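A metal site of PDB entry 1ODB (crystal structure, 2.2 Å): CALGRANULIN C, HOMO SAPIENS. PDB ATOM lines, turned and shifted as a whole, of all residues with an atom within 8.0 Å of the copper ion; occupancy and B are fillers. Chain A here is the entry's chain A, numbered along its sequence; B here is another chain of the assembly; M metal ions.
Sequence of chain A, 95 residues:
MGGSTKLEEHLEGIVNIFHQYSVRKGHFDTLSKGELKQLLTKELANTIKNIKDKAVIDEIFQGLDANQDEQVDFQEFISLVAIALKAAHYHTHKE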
ATOM      1  N   ALA A  88     -25.999 -23.648 -24.655  1.00  0.00           N
ATOM      2  CA  ALA A  88     -27.404 -23.598 -24.271  1.00  0.00           C
ATOM      3  C   ALA A  88     -27.756 -22.199 -23.788  1.00  0.00           C
ATOM      4  O   ALA A  88     -28.841 -21.730 -24.067  1.00  0.00           O
ATOM      5  CB  ALA A  88     -27.709 -24.627 -23.185  1.00  0.00           C
ATOM      6  N   HIS A  89     -26.836 -21.511 -23.110  1.00  0.00           N
ATOM      7  CA  HIS A  89     -27.078 -20.149 -22.661  1.00  0.00           C
ATOM      8  C   HIS A  89     -27.244 -19.196 -23.864  1.00  0.00           C
ATOM      9  O   HIS A  89     -28.204 -18.417 -23.937  1.00  0.00           O
ATOM     10  CB  HIS A  89     -25.993 -19.655 -21.694  1.00  0.00           C
ATOM     11  CG  HIS A  89     -26.275 -18.305 -21.123  1.00  0.00           C
ATOM     12  ND1 HIS A  89     -25.401 -17.253 -21.199  1.00  0.00           N
ATOM     13  CD2 HIS A  89     -27.374 -17.844 -20.486  1.00  0.00           C
ATOM     14  CE1 HIS A  89     -25.953 -16.188 -20.658  1.00  0.00           C
ATOM     15  NE2 HIS A  89     -27.157 -16.521 -20.200  1.00  0.00           N
ATOM     16  N   TYR A  90     -26.335 -19.317 -24.822  1.00  0.00           N
ATOM     17  CA  TYR A  90     -26.404 -18.573 -26.078  1.00  0.00           C
ATOM     18  C   TYR A  90     -27.708 -18.839 -26.841  1.00  0.00           C
ATOM     19  O   TYR A  90     -28.326 -17.913 -27.336  1.00  0.00           O
ATOM     20  CB  TYR A  90     -25.182 -18.916 -26.953  1.00  0.00           C
ATOM     21  CG  TYR A  90     -25.068 -18.121 -28.243  1.00  0.00           C
ATOM     22  CD1 TYR A  90     -24.459 -16.865 -28.257  1.00  0.00           C
ATOM     23  CD2 TYR A  90     -25.511 -18.648 -29.455  1.00  0.00           C
ATOM     24  CE1 TYR A  90     -24.328 -16.136 -29.445  1.00  0.00           C
ATOM     25  CE2 TYR A  90     -25.392 -17.927 -30.640  1.00  0.00           C
ATOM     26  CZ  TYR A  90     -24.809 -16.673 -30.627  1.00  0.00           C
ATOM     27  OH  TYR A  90     -24.683 -15.951 -31.783  1.00  0.00           O
ATOM     28  N   THR A  92     -30.638 -19.635 -25.731  1.00  0.00           N
ATOM     29  CA  THR A  92     -31.837 -19.080 -25.075  1.00  0.00           C
ATOM     30  C   THR A  92     -31.967 -17.614 -25.384  1.00  0.00           C
ATOM     31  O   THR A  92     -33.074 -17.099 -25.424  1.00  0.00           O
ATOM     32  CB  THR A  92     -31.890 -19.269 -23.507  1.00  0.00           C
ATOM     33  OG1 THR A  92     -30.971 -18.369 -22.868  1.00  0.00           O
ATOM     34  CG2 THR A  92     -31.439 -20.596 -23.070  1.00  0.00           C
ATOM     35  N   HIS A  93     -30.846 -16.922 -25.582  1.00  0.00           N
ATOM     36  CA  HIS A  93     -30.902 -15.510 -25.977  1.00  0.00           C
ATOM     37  C   HIS A  93     -30.895 -15.255 -27.486  1.00  0.00           C
ATOM     38  O   HIS A  93     -31.228 -14.157 -27.909  1.00  0.00           O
ATOM     39  CB  HIS A  93     -29.769 -14.717 -25.351  1.00  0.00           C
ATOM     40  CG  HIS A  93     -29.843 -14.652 -23.860  1.00  0.00           C
ATOM     41  ND1 HIS A  93     -30.884 -14.057 -23.190  1.00  0.00           N
ATOM     42  CD2 HIS A  93     -28.985 -15.087 -22.916  1.00  0.00           C
ATOM     43  CE1 HIS A  93     -30.678 -14.149 -21.888  1.00  0.00           C
ATOM     44  NE2 HIS A  93     -29.514 -14.745 -21.694  1.00  0.00           N
ATOM     45  N   VAL B  15     -29.548 -23.299 -16.807  1.00  0.00           N
ATOM     46  CA  VAL B  15     -29.630 -21.946 -17.358  1.00  0.00           C
ATOM     47  C   VAL B  15     -30.904 -21.265 -16.844  1.00  0.00           C
ATOM     48  O   VAL B  15     -30.863 -20.108 -16.420  1.00  0.00           O
ATOM     49  CB  VAL B  15     -29.674 -21.980 -18.896  1.00  0.00           C
ATOM     50  CG1 VAL B  15     -30.186 -20.653 -19.472  1.00  0.00           C
ATOM     51  CG2 VAL B  15     -28.324 -22.310 -19.431  1.00  0.00           C
ATOM     52  N   PHE B  18     -30.310 -20.197 -13.114  1.00  0.00           N
ATOM     53  CA  PHE B  18     -29.456 -19.032 -13.108  1.00  0.00           C
ATOM     54  C   PHE B  18     -30.280 -17.751 -13.325  1.00  0.00           C
ATOM     55  O   PHE B  18     -30.188 -16.780 -12.566  1.00  0.00           O
ATOM     56  CB  PHE B  18     -28.393 -19.177 -14.202  1.00  0.00           C
ATOM     57  CG  PHE B  18     -27.554 -17.957 -14.420  1.00  0.00           C
ATOM     58  CD1 PHE B  18     -26.472 -17.701 -13.607  1.00  0.00           C
ATOM     59  CD2 PHE B  18     -27.834 -17.076 -15.440  1.00  0.00           C
ATOM     60  CE1 PHE B  18     -25.668 -16.564 -13.803  1.00  0.00           C
ATOM     61  CE2 PHE B  18     -27.061 -15.932 -15.640  1.00  0.00           C
ATOM     62  CZ  PHE B  18     -25.988 -15.665 -14.835  1.00  0.00           C
ATOM     63  N   HIS B  19     -31.075 -17.779 -14.366  1.00  0.00           N
ATOM     64  CA  HIS B  19     -31.915 -16.633 -14.759  1.00  0.00           C
ATOM     65  C   HIS B  19     -32.961 -16.262 -13.730  1.00  0.00           C
ATOM     66  O   HIS B  19     -33.290 -15.106 -13.612  1.00  0.00           O
ATOM     67  CB  HIS B  19     -32.627 -16.909 -16.075  1.00  0.00           C
ATOM     68  CG  HIS B  19     -31.734 -16.800 -17.254  1.00  0.00           C
ATOM     69  ND1 HIS B  19     -31.967 -17.501 -18.424  1.00  0.00           N
ATOM     70  CD2 HIS B  19     -30.643 -16.033 -17.479  1.00  0.00           C
ATOM     71  CE1 HIS B  19     -31.053 -17.165 -19.310  1.00  0.00           C
ATOM     72  NE2 HIS B  19     -30.251 -16.270 -18.768  1.00  0.00           N
ATOM     73  N   SER B  22     -30.678 -14.160 -11.580  1.00  0.00           N
ATOM     74  CA  SER B  22     -29.927 -13.071 -12.214  1.00  0.00           C
ATOM     75  C   SER B  22     -30.814 -11.869 -12.547  1.00  0.00           C
ATOM     76  O   SER B  22     -30.341 -10.735 -12.526  1.00  0.00           O
ATOM     77  CB  SER B  22     -29.169 -13.544 -13.452  1.00  0.00           C
ATOM     78  OG  SER B  22     -30.020 -13.872 -14.529  1.00  0.00           O
ATOM     79  N   VAL B  23     -32.100 -12.110 -12.864  1.00  0.00           N
ATOM     80  CA  VAL B  23     -33.016 -11.016 -13.217  1.00  0.00           C
ATOM     81  C   VAL B  23     -33.483 -10.103 -12.115  1.00  0.00           C
ATOM     82  O   VAL B  23     -34.082  -9.069 -12.393  1.00  0.00           O
ATOM     83  CB  VAL B  23     -34.336 -11.511 -13.814  1.00  0.00           C
ATOM     84  CG1 VAL B  23     -34.053 -12.172 -15.060  1.00  0.00           C
ATOM     85  CG2 VAL B  23     -35.132 -12.436 -12.828  1.00  0.00           C
ATOM     86  N   HIS B  27     -28.010  -5.772 -13.388  1.00  0.00           N
ATOM     87  CA  HIS B  27     -27.944  -6.493 -14.655  1.00  0.00           C
ATOM     88  C   HIS B  27     -28.778  -7.769 -14.600  1.00  0.00           C
ATOM     89  O   HIS B  27     -28.607  -8.597 -13.701  1.00  0.00           O
ATOM     90  CB  HIS B  27     -26.493  -6.869 -15.016  1.00  0.00           C
ATOM     91  CG  HIS B  27     -26.280  -7.084 -16.481  1.00  0.00           C
ATOM     92  ND1 HIS B  27     -25.834  -6.083 -17.320  1.00  0.00           N
ATOM     93  CD2 HIS B  27     -26.495  -8.165 -17.260  1.00  0.00           C
ATOM     94  CE1 HIS B  27     -25.748  -6.559 -18.560  1.00  0.00           C
ATOM     95  NE2 HIS B  27     -26.146  -7.818 -18.542  1.00  0.00           N
ATOM     96  N   PHE B  28     -29.648  -7.932 -15.598  1.00  0.00           N
ATOM     97  CA  PHE B  28     -30.586  -9.053 -15.649  1.00  0.00           C
ATOM     98  C   PHE B  28     -29.897 -10.404 -15.840  1.00  0.00           C
ATOM     99  O   PHE B  28     -30.488 -11.447 -15.582  1.00  0.00           O
ATOM    100  CB  PHE B  28     -31.610  -8.838 -16.793  1.00  0.00           C
ATOM    101  CG  PHE B  28     -31.038  -9.047 -18.153  1.00  0.00           C
ATOM    102  CD1 PHE B  28     -31.115 -10.284 -18.761  1.00  0.00           C
ATOM    103  CD2 PHE B  28     -30.392  -8.021 -18.823  1.00  0.00           C
ATOM    104  CE1 PHE B  28     -30.566 -10.501 -20.024  1.00  0.00           C
ATOM    105  CE2 PHE B  28     -29.850  -8.225 -20.084  1.00  0.00           C
ATOM    106  CZ  PHE B  28     -29.939  -9.470 -20.690  1.00  0.00           C
ATOM    107  N   ASP B  29     -28.627 -10.368 -16.259  1.00  0.00           N
ATOM    108  CA  ASP B  29     -27.909 -11.545 -16.740  1.00  0.00           C
ATOM    109  C   ASP B  29     -26.632 -11.825 -15.959  1.00  0.00           C
ATOM    110  O   ASP B  29     -25.818 -12.657 -16.363  1.00  0.00           O
ATOM    111  CB  ASP B  29     -27.580 -11.366 -18.227  1.00  0.00           C
ATOM    112  CG  ASP B  29     -27.648 -12.663 -19.019  1.00  0.00           C
ATOM    113  OD1 ASP B  29     -28.303 -13.646 -18.585  1.00  0.00           O
ATOM    114  OD2 ASP B  29     -27.071 -12.788 -20.107  1.00  0.00           O
ATOM    115  N   THR B  30     -26.452 -11.128 -14.838  1.00  0.00           N
ATOM    116  CA  THR B  30     -25.400 -11.458 -13.881  1.00  0.00           C
ATOM    117  C   THR B  30     -25.959 -11.514 -12.471  1.00  0.00           C
ATOM    118  O   THR B  30     -27.065 -11.022 -12.192  1.00  0.00           O
ATOM    119  CB  THR B  30     -24.236 -10.477 -13.947  1.00  0.00           C
ATOM    120  OG1 THR B  30     -24.651  -9.172 -13.508  1.00  0.00           O
ATOM    121  CG2 THR B  30     -23.743 -10.267 -15.389  1.00  0.00           C
ATOM    122  N   PHE B  74     -22.462 -15.376 -16.438  1.00  0.00           N
ATOM    123  CA  PHE B  74     -22.781 -16.776 -16.678  1.00  0.00           C
ATOM    124  C   PHE B  74     -21.539 -17.642 -16.807  1.00  0.00           C
ATOM    125  O   PHE B  74     -21.487 -18.717 -16.200  1.00  0.00           O
ATOM    126  CB  PHE B  74     -23.678 -17.003 -17.882  1.00  0.00           C
ATOM    127  CG  PHE B  74     -24.192 -18.431 -17.975  1.00  0.00           C
ATOM    128  CD1 PHE B  74     -25.221 -18.860 -17.141  1.00  0.00           C
ATOM    129  CD2 PHE B  74     -23.625 -19.345 -18.853  1.00  0.00           C
ATOM    130  CE1 PHE B  74     -25.673 -20.195 -17.190  1.00  0.00           C
ATOM    131  CE2 PHE B  74     -24.072 -20.652 -18.914  1.00  0.00           C
ATOM    132  CZ  PHE B  74     -25.102 -21.071 -18.092  1.00  0.00           C
HETATM  133 CU    CU M   1     -28.686 -15.261 -19.776  1.00  0.00          CU
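The backbone carbonyl oxygen (O) of His 89 sits at hydrogen-bond distance from the side-chain hydroxyl (OG1) of Thr 92 (3.0 Å). ND1 of His 19 of chain B lies within hydrogen-bond range of O of Val 15 of chain B.
The copper ion is bound by a ring nitrogen (NE2) of His 89, the side-chain carboxylate (OD1) of Asp 29 of chain B, a ring nitrogen (NE2) of His 19 of chain B and a ring nitrogen (NE2) of His 93.
Of the 15 residues printed, 4 come within 4 Å of the copper ion. Along chain A the residues within 4 Å of the copper ion span positions 89 to 93.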
